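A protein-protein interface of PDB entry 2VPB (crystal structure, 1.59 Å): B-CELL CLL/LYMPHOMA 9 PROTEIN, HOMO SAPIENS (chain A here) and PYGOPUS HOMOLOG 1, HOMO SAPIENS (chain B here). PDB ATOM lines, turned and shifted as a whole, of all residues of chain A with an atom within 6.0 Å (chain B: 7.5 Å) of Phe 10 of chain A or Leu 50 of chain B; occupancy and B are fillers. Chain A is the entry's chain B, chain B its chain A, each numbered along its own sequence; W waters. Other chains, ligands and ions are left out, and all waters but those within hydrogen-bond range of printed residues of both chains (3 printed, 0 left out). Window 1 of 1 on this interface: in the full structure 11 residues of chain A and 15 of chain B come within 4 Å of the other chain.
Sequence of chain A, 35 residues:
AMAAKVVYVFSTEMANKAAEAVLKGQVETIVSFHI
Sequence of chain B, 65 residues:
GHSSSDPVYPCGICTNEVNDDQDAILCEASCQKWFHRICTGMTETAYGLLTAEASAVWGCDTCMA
Of the 23 printed residues of chain B, 12 touch a printed residue of chain A.
Hydrophobic or aromatic side chains of chain B that line the printed part of chain A: Ala 29, Met 42, Ala 46, Leu 49, Leu 50, Ala 56, Val 57, Trp 58 and Met 64.
Among the printed residues, 24 pairs touch across the chains.
Among the printed residues, no Asp or Glu carboxylate lies within 4 Å of a Lys or Arg side-chain nitrogen of the other chain.
Of the printed residues of chain B, Val 9 of chain A touches Ala 29 (3.9 Å), Val 57 (3.5 Å), Gly 59 (3.9 Å) and Met 64 (3.5 Å).
Of chain B, only Leu 50, Ala 56, Val 57, Trp 58 and Gly 59 come within 4 Å of Phe 10 of chain A.
Phe 33 of chain A touches none of the printed residues of chain B.
Of the printed residues of chain A, Glu 53 of chain B touches Val 31 (3.7 Å).
Of the printed residues of chain A, Ser 55 of chain B touches Tyr 8 and Val 31.
Of the printed residues of chain A, Met 64 of chain B touches Val 9 (3.5 Å) and Ser 11 (3.97 Å).
The nearest residue of chain B that does not touch Phe 10 of chain A is Met 64 of chain B (4.4 Å).
The nearest residue of chain A that does not touch Leu 50 of chain B is Ala 15 of chain A (4.2 Å).
The nearest printed residue of chain A that does not touch Trp 58 of chain B is Val 9 of chain A (4.1 Å).
SD of Met 42 of chain B sits close to N of Tyr 47 of chain B, 3.7 Å away.
The backbone NH (N) of Met 14 of chain A sits at hydrogen-bond distance from the side-chain hydroxyl (OG) of Ser 11 of chain A, 3.2 Å away.
The side-chain carboxylate of Glu 53 of chain B sits at hydrogen-bond distance from the side-chain hydroxyl of Ser 55 of chain B, at 2.7 Å.
Among the printed residues, pairs that only touch across the chains: Phe 10 of chain A with Trp 58 of chain B (3.2 Å), Tyr 8 of chain A with Ala 56 of chain B (3.4 Å), Thr 12 of chain A with Met 42 of chain B (3.4 Å), Val 9 of chain A with Met 64 of chain B (3.5 Å), Val 9 of chain A with Val 57 of chain B (3.5 Å), Ala 15 of chain A with Ala 46 of chain B (3.5 Å), Phe 10 of chain A with Ala 56 of chain B (3.6 Å), Val 31 of chain A with Ser 55 of chain B (3.7 Å), Ile 30 of chain A with Leu 50 of chain B (3.7 Å), Ser 11 of chain A with Gly 59 of chain B (3.7 Å), Val 31 of chain A with Glu 53 of chain B (3.7 Å), Phe 10 of chain A with Leu 50 of chain B (3.8 Å), Ile 30 of chain A with Leu 49 of chain B (3.9 Å), Val 9 of chain A with Gly 59 of chain B (3.9 Å), Ala 15 of chain A with Met 42 of chain B (3.9 Å), Val 9 of chain A with Ala 29 of chain B (3.9 Å), Val 31 of chain A with Ala 56 of chain B (3.96 Å), Ser 11 of chain A with Met 64 of chain B (3.97 Å) and Ser 11 of chain A with Trp 58 of chain B (3.99 Å).
Water W3 lies within hydrogen-bond range of the side-chain carboxylate (OD1) of Asp 61 of chain B (2.6 Å), the backbone carbonyl oxygen (O) of Gly 59 of chain B (2.7 Å), the backbone NH (N) of Thr 12 of chain A (2.8 Å) and the indole nitrogen (NE1) of Trp 58 of chain B (3.5 Å).
Water W1 lies within hydrogen-bond range of the side-chain hydroxyl (OG1) of Thr 12 of chain A (2.7 Å) and the side-chain carboxylate (OD1) of Asp 61 of chain B (3.1 Å).
Water W2 bridges the backbone carbonyl oxygen of Ala 46 of chain B (3.0 Å) and the backbone carbonyl oxygen of Ala 15 of chain A (3.1 Å).
The backbone NH of Val 57 of chain B is in hydrogen-bond range of the backbone carbonyl oxygen of Tyr 8 of chain A (2.8 Å).
The backbone NH (N) of Gly 59 of chain B sits at hydrogen-bond distance from the backbone carbonyl oxygen (O) of Phe 10 of chain A, at 2.9 Å.
The backbone NH (N) of Phe 10 of chain A lies within hydrogen-bond range of the backbone carbonyl oxygen (O) of Val 57 of chain B (2.8 Å).
The indole nitrogen (NE1) of Trp 58 of chain B lies within hydrogen-bond range of the side-chain hydroxyl (OG1) of Thr 12 of chain A.
O of Ser 55 of chain B lies within hydrogen-bond range of N of Tyr 8 of chain A, 2.8 Å away.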
ATOM      1  N   TYR A   8       5.838   5.042 -11.919  1.00  0.00           N
ATOM      2  CA  TYR A   8       5.994   6.484 -11.765  1.00  0.00           C
ATOM      3  C   TYR A   8       7.441   6.827 -11.460  1.00  0.00           C
ATOM      4  O   TYR A   8       8.073   6.201 -10.606  1.00  0.00           O
ATOM      5  CB  TYR A   8       5.055   6.983 -10.671  1.00  0.00           C
ATOM      6  CG  TYR A   8       3.624   6.817 -11.088  1.00  0.00           C
ATOM      7  CD1 TYR A   8       3.079   7.658 -12.059  1.00  0.00           C
ATOM      8  CD2 TYR A   8       2.828   5.804 -10.550  1.00  0.00           C
ATOM      9  CE1 TYR A   8       1.775   7.502 -12.484  1.00  0.00           C
ATOM     10  CE2 TYR A   8       1.493   5.648 -10.977  1.00  0.00           C
ATOM     11  CZ  TYR A   8       0.991   6.509 -11.939  1.00  0.00           C
ATOM     12  OH  TYR A   8      -0.316   6.381 -12.374  1.00  0.00           O
ATOM     13  N   VAL A   9       7.968   7.813 -12.179  1.00  0.00           N
ATOM     14  CA  VAL A   9       9.367   8.217 -12.058  1.00  0.00           C
ATOM     15  C   VAL A   9       9.410   9.583 -11.374  1.00  0.00           C
ATOM     16  O   VAL A   9       8.953  10.581 -11.934  1.00  0.00           O
ATOM     17  CB  VAL A   9      10.072   8.251 -13.438  1.00  0.00           C
ATOM     18  CG1 VAL A   9      11.564   8.513 -13.278  1.00  0.00           C
ATOM     19  CG2 VAL A   9       9.849   6.922 -14.189  1.00  0.00           C
ATOM     20  N   PHE A  10       9.916   9.600 -10.139  1.00  0.00           N
ATOM     21  CA  PHE A  10       9.977  10.825  -9.336  1.00  0.00           C
ATOM     22  C   PHE A  10      11.367  11.474  -9.405  1.00  0.00           C
ATOM     23  O   PHE A  10      12.383  10.811  -9.158  1.00  0.00           O
ATOM     24  CB  PHE A  10       9.747  10.482  -7.854  1.00  0.00           C
ATOM     25  CG  PHE A  10       8.330  10.113  -7.495  1.00  0.00           C
ATOM     26  CD1 PHE A  10       7.533  10.991  -6.773  1.00  0.00           C
ATOM     27  CD2 PHE A  10       7.811   8.869  -7.828  1.00  0.00           C
ATOM     28  CE1 PHE A  10       6.216  10.666  -6.423  1.00  0.00           C
ATOM     29  CE2 PHE A  10       6.506   8.522  -7.475  1.00  0.00           C
ATOM     30  CZ  PHE A  10       5.702   9.430  -6.771  1.00  0.00           C
ATOM     31  N   SER A  11      11.419  12.777  -9.699  1.00  0.00           N
ATOM     32  CA  SER A  11      12.615  13.548  -9.399  1.00  0.00           C
ATOM     33  C   SER A  11      12.798  13.647  -7.886  1.00  0.00           C
ATOM     34  O   SER A  11      11.880  13.348  -7.107  1.00  0.00           O
ATOM     35  CB  SER A  11      12.516  14.970  -9.973  1.00  0.00           C
ATOM     36  OG  SER A  11      11.446  15.674  -9.366  1.00  0.00           O
ATOM     37  N   THR A  12      13.979  14.089  -7.470  1.00  0.00           N
ATOM     38  CA  THR A  12      14.211  14.335  -6.042  1.00  0.00           C
ATOM     39  C   THR A  12      13.194  15.334  -5.488  1.00  0.00           C
ATOM     40  O   THR A  12      12.631  15.118  -4.416  1.00  0.00           O
ATOM     41  CB  THR A  12      15.618  14.831  -5.810  1.00  0.00           C
ATOM     42  OG1 THR A  12      16.535  13.792  -6.168  1.00  0.00           O
ATOM     43  CG2 THR A  12      15.821  15.184  -4.361  1.00  0.00           C
ATOM     44  N   MET A  14      10.128  15.953  -6.492  1.00  0.00           N
ATOM     45  CA  MET A  14       8.797  15.392  -6.361  1.00  0.00           C
ATOM     46  C   MET A  14       8.729  14.239  -5.348  1.00  0.00           C
ATOM     47  O   MET A  14       7.681  14.019  -4.737  1.00  0.00           O
ATOM     48  CB  MET A  14       8.216  15.035  -7.738  1.00  0.00           C
ATOM     49  CG  MET A  14       8.138  16.257  -8.675  1.00  0.00           C
ATOM     50  SD  MET A  14       7.123  17.614  -8.042  1.00  0.00           S
ATOM     51  CE  MET A  14       5.525  16.822  -8.037  1.00  0.00           C
ATOM     52  N   ALA A  15       9.841  13.535  -5.135  1.00  0.00           N
ATOM     53  CA  ALA A  15       9.907  12.564  -4.040  1.00  0.00           C
ATOM     54  C   ALA A  15       9.788  13.261  -2.693  1.00  0.00           C
ATOM     55  O   ALA A  15       9.033  12.818  -1.825  1.00  0.00           O
ATOM     56  CB  ALA A  15      11.190  11.717  -4.114  1.00  0.00           C
ATOM     57  N   ALA A  18       6.221  14.613  -2.313  1.00  0.00           N
ATOM     58  CA  ALA A  18       5.244  13.563  -2.052  1.00  0.00           C
ATOM     59  C   ALA A  18       5.362  13.086  -0.606  1.00  0.00           C
ATOM     60  O   ALA A  18       4.356  12.831   0.020  1.00  0.00           O
ATOM     61  CB  ALA A  18       5.418  12.406  -3.020  1.00  0.00           C
ATOM     62  N   ILE A  30       2.699   8.025  -1.524  1.00  0.00           N
ATOM     63  CA  ILE A  30       3.366   8.926  -2.470  1.00  0.00           C
ATOM     64  C   ILE A  30       2.860   8.756  -3.907  1.00  0.00           C
ATOM     65  O   ILE A  30       3.174   9.589  -4.762  1.00  0.00           O
ATOM     66  CB  ILE A  30       4.922   8.797  -2.427  1.00  0.00           C
ATOM     67  CG1 ILE A  30       5.392   7.373  -2.820  1.00  0.00           C
ATOM     68  CG2 ILE A  30       5.465   9.202  -1.039  1.00  0.00           C
ATOM     69  CD1 ILE A  30       6.844   7.300  -3.176  1.00  0.00           C
ATOM     70  N   VAL A  31       2.084   7.702  -4.181  1.00  0.00           N
ATOM     71  CA  VAL A  31       1.495   7.525  -5.522  1.00  0.00           C
ATOM     72  C   VAL A  31      -0.033   7.651  -5.514  1.00  0.00           C
ATOM     73  O   VAL A  31      -0.706   7.241  -6.468  1.00  0.00           O
ATOM     74  CB  VAL A  31       1.943   6.197  -6.211  1.00  0.00           C
ATOM     75  CG1 VAL A  31       3.440   6.231  -6.557  1.00  0.00           C
ATOM     76  CG2 VAL A  31       1.605   4.992  -5.339  1.00  0.00           C
ATOM     77  N   PHE A  33      -2.215   9.712  -6.414  1.00  0.00           N
ATOM     78  CA  PHE A  33      -2.517  10.891  -7.237  1.00  0.00           C
ATOM     79  C   PHE A  33      -4.011  11.154  -7.250  1.00  0.00           C
ATOM     80  O   PHE A  33      -4.812  10.226  -7.160  1.00  0.00           O
ATOM     81  CB  PHE A  33      -1.991  10.725  -8.660  1.00  0.00           C
ATOM     82  CG  PHE A  33      -0.539  10.390  -8.719  1.00  0.00           C
ATOM     83  CD1 PHE A  33       0.421  11.345  -8.434  1.00  0.00           C
ATOM     84  CD2 PHE A  33      -0.132   9.105  -9.053  1.00  0.00           C
ATOM     85  CE1 PHE A  33       1.788  11.018  -8.473  1.00  0.00           C
ATOM     86  CE2 PHE A  33       1.222   8.779  -9.109  1.00  0.00           C
ATOM     87  CZ  PHE A  33       2.176   9.736  -8.818  1.00  0.00           C
ATOM     88  N   ILE B  25      20.763   5.068  -4.232  1.00  0.00           N
ATOM     89  CA  ILE B  25      19.626   5.165  -5.144  1.00  0.00           C
ATOM     90  C   ILE B  25      20.053   5.063  -6.612  1.00  0.00           C
ATOM     91  O   ILE B  25      21.074   5.616  -7.012  1.00  0.00           O
ATOM     92  CB  ILE B  25      18.782   6.432  -4.841  1.00  0.00           C
ATOM     93  CG1 ILE B  25      17.418   6.349  -5.523  1.00  0.00           C
ATOM     94  CG2 ILE B  25      19.542   7.717  -5.176  1.00  0.00           C
ATOM     95  CD1 ILE B  25      16.363   7.160  -4.831  1.00  0.00           C
ATOM     96  N   LEU B  26      19.278   4.305  -7.393  1.00  0.00           N
ATOM     97  CA  LEU B  26      19.574   4.054  -8.785  1.00  0.00           C
ATOM     98  C   LEU B  26      18.680   4.930  -9.644  1.00  0.00           C
ATOM     99  O   LEU B  26      17.465   4.987  -9.427  1.00  0.00           O
ATOM    100  CB  LEU B  26      19.279   2.579  -9.103  1.00  0.00           C
ATOM    101  CG  LEU B  26      19.435   2.115 -10.552  1.00  0.00           C
ATOM    102  CD1 LEU B  26      20.883   2.150 -11.008  1.00  0.00           C
ATOM    103  CD2 LEU B  26      18.847   0.714 -10.722  1.00  0.00           C
ATOM    104  N   ALA B  29      15.250   6.412 -14.604  1.00  0.00           N
ATOM    105  CA  ALA B  29      14.688   7.175 -15.711  1.00  0.00           C
ATOM    106  C   ALA B  29      15.398   6.769 -17.000  1.00  0.00           C
ATOM    107  O   ALA B  29      14.742   6.550 -18.023  1.00  0.00           O
ATOM    108  CB  ALA B  29      14.817   8.668 -15.470  1.00  0.00           C
ATOM    109  N   MET B  42      17.546  14.134  -1.608  1.00  0.00           N
ATOM    110  CA  MET B  42      16.341  13.439  -1.127  1.00  0.00           C
ATOM    111  C   MET B  42      16.400  13.242   0.385  1.00  0.00           C
ATOM    112  O   MET B  42      17.431  12.823   0.918  1.00  0.00           O
ATOM    113  CB  MET B  42      16.205  12.095  -1.835  1.00  0.00           C
ATOM    114  CG  MET B  42      14.892  11.427  -1.574  1.00  0.00           C
ATOM    115  SD  MET B  42      14.791   9.814  -2.377  1.00  0.00           S
ATOM    116  CE  MET B  42      14.827  10.316  -4.083  1.00  0.00           C
ATOM    117  N   GLU B  44      15.683  11.435   4.050  1.00  0.00           N
ATOM    118  CA  GLU B  44      15.656  10.026   4.446  1.00  0.00           C
ATOM    119  C   GLU B  44      14.222   9.498   4.413  1.00  0.00           C
ATOM    120  O   GLU B  44      13.993   8.359   4.019  1.00  0.00           O
ATOM    121  CB  GLU B  44      16.217   9.858   5.872  1.00  0.00           C
ATOM    122  CG  GLU B  44      17.705  10.141   5.988  1.00  0.00           C
ATOM    123  CD  GLU B  44      18.308   9.639   7.288  1.00  0.00           C
ATOM    124  OE1 GLU B  44      18.209   8.426   7.585  1.00  0.00           O
ATOM    125  OE2 GLU B  44      18.911  10.463   7.999  1.00  0.00           O
ATOM    126  N   THR B  45      13.253  10.320   4.814  1.00  0.00           N
ATOM    127  CA  THR B  45      11.858   9.875   4.808  1.00  0.00           C
ATOM    128  C   THR B  45      11.350   9.659   3.393  1.00  0.00           C
ATOM    129  O   THR B  45      10.699   8.647   3.122  1.00  0.00           O
ATOM    130  CB  THR B  45      10.964  10.865   5.581  1.00  0.00           C
ATOM    131  OG1 THR B  45      11.438  10.903   6.931  1.00  0.00           O
ATOM    132  CG2 THR B  45       9.495  10.426   5.562  1.00  0.00           C
ATOM    133  N   ALA B  46      11.669  10.579   2.485  1.00  0.00           N
ATOM    134  CA  ALA B  46      11.271  10.397   1.084  1.00  0.00           C
ATOM    135  C   ALA B  46      11.906   9.162   0.466  1.00  0.00           C
ATOM    136  O   ALA B  46      11.257   8.445  -0.303  1.00  0.00           O
ATOM    137  CB  ALA B  46      11.618  11.639   0.258  1.00  0.00           C
ATOM    138  N   TYR B  47      13.161   8.900   0.821  1.00  0.00           N
ATOM    139  CA  TYR B  47      13.866   7.725   0.345  1.00  0.00           C
ATOM    140  C   TYR B  47      13.203   6.444   0.847  1.00  0.00           C
ATOM    141  O   TYR B  47      12.999   5.490   0.084  1.00  0.00           O
ATOM    142  CB  TYR B  47      15.320   7.809   0.809  1.00  0.00           C
ATOM    143  CG  TYR B  47      16.177   6.619   0.489  1.00  0.00           C
ATOM    144  CD1 TYR B  47      16.748   6.458  -0.776  1.00  0.00           C
ATOM    145  CD2 TYR B  47      16.421   5.657   1.455  1.00  0.00           C
ATOM    146  CE1 TYR B  47      17.561   5.353  -1.066  1.00  0.00           C
ATOM    147  CE2 TYR B  47      17.233   4.561   1.183  1.00  0.00           C
ATOM    148  CZ  TYR B  47      17.784   4.413  -0.070  1.00  0.00           C
ATOM    149  OH  TYR B  47      18.573   3.305  -0.310  1.00  0.00           O
ATOM    150  N   GLY B  48      12.857   6.427   2.131  1.00  0.00           N
ATOM    151  CA  GLY B  48      12.171   5.260   2.692  1.00  0.00           C
ATOM    152  C   GLY B  48      10.844   4.972   2.001  1.00  0.00           C
ATOM    153  O   GLY B  48      10.520   3.815   1.694  1.00  0.00           O
ATOM    154  N   LEU B  49      10.072   6.030   1.738  1.00  0.00           N
ATOM    155  CA  LEU B  49       8.771   5.856   1.094  1.00  0.00           C
ATOM    156  C   LEU B  49       8.907   5.415  -0.354  1.00  0.00           C
ATOM    157  O   LEU B  49       8.163   4.545  -0.826  1.00  0.00           O
ATOM    158  CB  LEU B  49       7.955   7.155   1.179  1.00  0.00           C
ATOM    159  CG  LEU B  49       7.539   7.587   2.591  1.00  0.00           C
ATOM    160  CD1 LEU B  49       6.925   8.973   2.549  1.00  0.00           C
ATOM    161  CD2 LEU B  49       6.579   6.582   3.203  1.00  0.00           C
ATOM    162  N   LEU B  50       9.854   6.010  -1.073  1.00  0.00           N
ATOM    163  CA  LEU B  50      10.045   5.666  -2.463  1.00  0.00           C
ATOM    164  C   LEU B  50      10.545   4.230  -2.608  1.00  0.00           C
ATOM    165  O   LEU B  50      10.074   3.488  -3.469  1.00  0.00           O
ATOM    166  CB  LEU B  50      10.999   6.666  -3.121  1.00  0.00           C
ATOM    167  CG  LEU B  50      11.198   6.641  -4.633  1.00  0.00           C
ATOM    168  CD1 LEU B  50       9.912   6.808  -5.382  1.00  0.00           C
ATOM    169  CD2 LEU B  50      12.143   7.772  -5.003  1.00  0.00           C
ATOM    170  N   THR B  51      11.466   3.812  -1.746  1.00  0.00           N
ATOM    171  CA  THR B  51      12.047   2.481  -1.919  1.00  0.00           C
ATOM    172  C   THR B  51      11.050   1.390  -1.492  1.00  0.00           C
ATOM    173  O   THR B  51      11.161   0.242  -1.933  1.00  0.00           O
ATOM    174  CB  THR B  51      13.435   2.379  -1.247  1.00  0.00           C
ATOM    175  OG1 THR B  51      13.323   2.752   0.117  1.00  0.00           O
ATOM    176  CG2 THR B  51      14.404   3.320  -1.927  1.00  0.00           C
ATOM    177  N   ALA B  52      10.048   1.760  -0.695  1.00  0.00           N
ATOM    178  CA  ALA B  52       8.993   0.826  -0.259  1.00  0.00           C
ATOM    179  C   ALA B  52       7.844   0.693  -1.258  1.00  0.00           C
ATOM    180  O   ALA B  52       7.089  -0.290  -1.237  1.00  0.00           O
ATOM    181  CB  ALA B  52       8.447   1.236   1.081  1.00  0.00           C
ATOM    182  N   GLU B  53       7.682   1.693  -2.109  1.00  0.00           N
ATOM    183  CA  GLU B  53       6.577   1.692  -3.055  1.00  0.00           C
ATOM    184  C   GLU B  53       7.003   1.060  -4.368  1.00  0.00           C
ATOM    185  O   GLU B  53       7.872   1.573  -5.073  1.00  0.00           O
ATOM    186  CB  GLU B  53       6.068   3.121  -3.270  1.00  0.00           C
ATOM    187  CG  GLU B  53       5.018   3.230  -4.381  1.00  0.00           C
ATOM    188  CD  GLU B  53       3.844   2.262  -4.214  1.00  0.00           C
ATOM    189  OE1 GLU B  53       3.230   2.239  -3.120  1.00  0.00           O
ATOM    190  OE2 GLU B  53       3.528   1.534  -5.192  1.00  0.00           O
ATOM    191  N   ALA B  54       6.396  -0.074  -4.705  1.00  0.00           N
ATOM    192  CA  ALA B  54       6.821  -0.814  -5.880  1.00  0.00           C
ATOM    193  C   ALA B  54       6.587  -0.080  -7.213  1.00  0.00           C
ATOM    194  O   ALA B  54       7.329  -0.289  -8.184  1.00  0.00           O
ATOM    195  CB  ALA B  54       6.152  -2.181  -5.904  1.00  0.00           C
ATOM    196  N   SER B  55       5.579   0.790  -7.250  1.00  0.00           N
ATOM    197  CA  SER B  55       5.218   1.479  -8.496  1.00  0.00           C
ATOM    198  C   SER B  55       5.941   2.802  -8.678  1.00  0.00           C
ATOM    199  O   SER B  55       5.623   3.550  -9.593  1.00  0.00           O
ATOM    200  CB  SER B  55       3.706   1.715  -8.579  1.00  0.00           C
ATOM    201  OG  SER B  55       3.273   2.685  -7.634  1.00  0.00           O
ATOM    202  N   ALA B  56       6.916   3.074  -7.814  1.00  0.00           N
ATOM    203  CA  ALA B  56       7.605   4.365  -7.821  1.00  0.00           C
ATOM    204  C   ALA B  56       9.099   4.161  -7.877  1.00  0.00           C
ATOM    205  O   ALA B  56       9.652   3.395  -7.094  1.00  0.00           O
ATOM    206  CB  ALA B  56       7.248   5.155  -6.582  1.00  0.00           C
ATOM    207  N   VAL B  57       9.751   4.868  -8.790  1.00  0.00           N
ATOM    208  CA  VAL B  57      11.198   4.828  -8.897  1.00  0.00           C
ATOM    209  C   VAL B  57      11.685   6.261  -9.001  1.00  0.00           C
ATOM    210  O   VAL B  57      10.883   7.196  -9.049  1.00  0.00           O
ATOM    211  CB  VAL B  57      11.679   3.977 -10.107  1.00  0.00           C
ATOM    212  CG1 VAL B  57      11.172   2.559  -9.963  1.00  0.00           C
ATOM    213  CG2 VAL B  57      11.235   4.590 -11.422  1.00  0.00           C
ATOM    214  N   TRP B  58      12.999   6.423  -8.967  1.00  0.00           N
ATOM    215  CA  TRP B  58      13.616   7.743  -8.965  1.00  0.00           C
ATOM    216  C   TRP B  58      14.339   7.988 -10.280  1.00  0.00           C
ATOM    217  O   TRP B  58      14.899   7.061 -10.888  1.00  0.00           O
ATOM    218  CB  TRP B  58      14.606   7.840  -7.795  1.00  0.00           C
ATOM    219  CG  TRP B  58      15.397   9.120  -7.734  1.00  0.00           C
ATOM    220  CD1 TRP B  58      14.967  10.349  -7.321  1.00  0.00           C
ATOM    221  CD2 TRP B  58      16.767   9.272  -8.101  1.00  0.00           C
ATOM    222  NE1 TRP B  58      15.996  11.263  -7.412  1.00  0.00           N
ATOM    223  CE2 TRP B  58      17.115  10.622  -7.880  1.00  0.00           C
ATOM    224  CE3 TRP B  58      17.742   8.390  -8.589  1.00  0.00           C
ATOM    225  CZ2 TRP B  58      18.402  11.118  -8.141  1.00  0.00           C
ATOM    226  CZ3 TRP B  58      19.019   8.879  -8.848  1.00  0.00           C
ATOM    227  CH2 TRP B  58      19.339  10.232  -8.620  1.00  0.00           C
ATOM    228  N   GLY B  59      14.353   9.252 -10.687  1.00  0.00           N
ATOM    229  CA  GLY B  59      15.140   9.698 -11.830  1.00  0.00           C
ATOM    230  C   GLY B  59      16.011  10.861 -11.420  1.00  0.00           C
ATOM    231  O   GLY B  59      15.569  11.777 -10.717  1.00  0.00           O
ATOM    232  N   CYS B  60      17.257  10.853 -11.886  1.00  0.00           N
ATOM    233  CA  CYS B  60      18.184  11.927 -11.560  1.00  0.00           C
ATOM    234  C   CYS B  60      17.816  13.230 -12.276  1.00  0.00           C
ATOM    235  O   CYS B  60      17.047  13.215 -13.234  1.00  0.00           O
ATOM    236  CB  CYS B  60      19.632  11.518 -11.841  1.00  0.00           C
ATOM    237  SG  CYS B  60      20.099  11.577 -13.611  1.00  0.00           S
ATOM    238  N   ASP B  61      18.358  14.344 -11.795  1.00  0.00           N
ATOM    239  CA  ASP B  61      18.039  15.654 -12.343  1.00  0.00           C
ATOM    240  C   ASP B  61      18.369  15.716 -13.835  1.00  0.00           C
ATOM    241  O   ASP B  61      17.627  16.319 -14.612  1.00  0.00           O
ATOM    242  CB  ASP B  61      18.787  16.752 -11.579  1.00  0.00           C
ATOM    243  CG  ASP B  61      18.304  16.910 -10.132  1.00  0.00           C
ATOM    244  OD1 ASP B  61      17.255  16.330  -9.768  1.00  0.00           O
ATOM    245  OD2 ASP B  61      18.971  17.640  -9.365  1.00  0.00           O
ATOM    246  N   MET B  64      15.773  13.620 -15.840  1.00  0.00           N
ATOM    247  CA  MET B  64      14.443  14.202 -15.703  1.00  0.00           C
ATOM    248  C   MET B  64      14.318  15.542 -16.424  1.00  0.00           C
ATOM    249  O   MET B  64      13.215  15.928 -16.819  1.00  0.00           O
ATOM    250  CB  MET B  64      14.055  14.362 -14.227  1.00  0.00           C
ATOM    251  CG  MET B  64      13.895  13.052 -13.459  1.00  0.00           C
ATOM    252  SD  MET B  64      12.725  11.903 -14.194  1.00  0.00           S
ATOM    253  CE  MET B  64      11.160  12.605 -13.660  1.00  0.00           C
HETATM  254  O   HOH W   1      18.610  15.135  -7.294  1.00  0.00           O
HETATM  255  O   HOH W   2       8.897   9.754  -1.504  1.00  0.00           O
HETATM  256  O   HOH W   3      15.982  14.111  -9.390  1.00  0.00           O
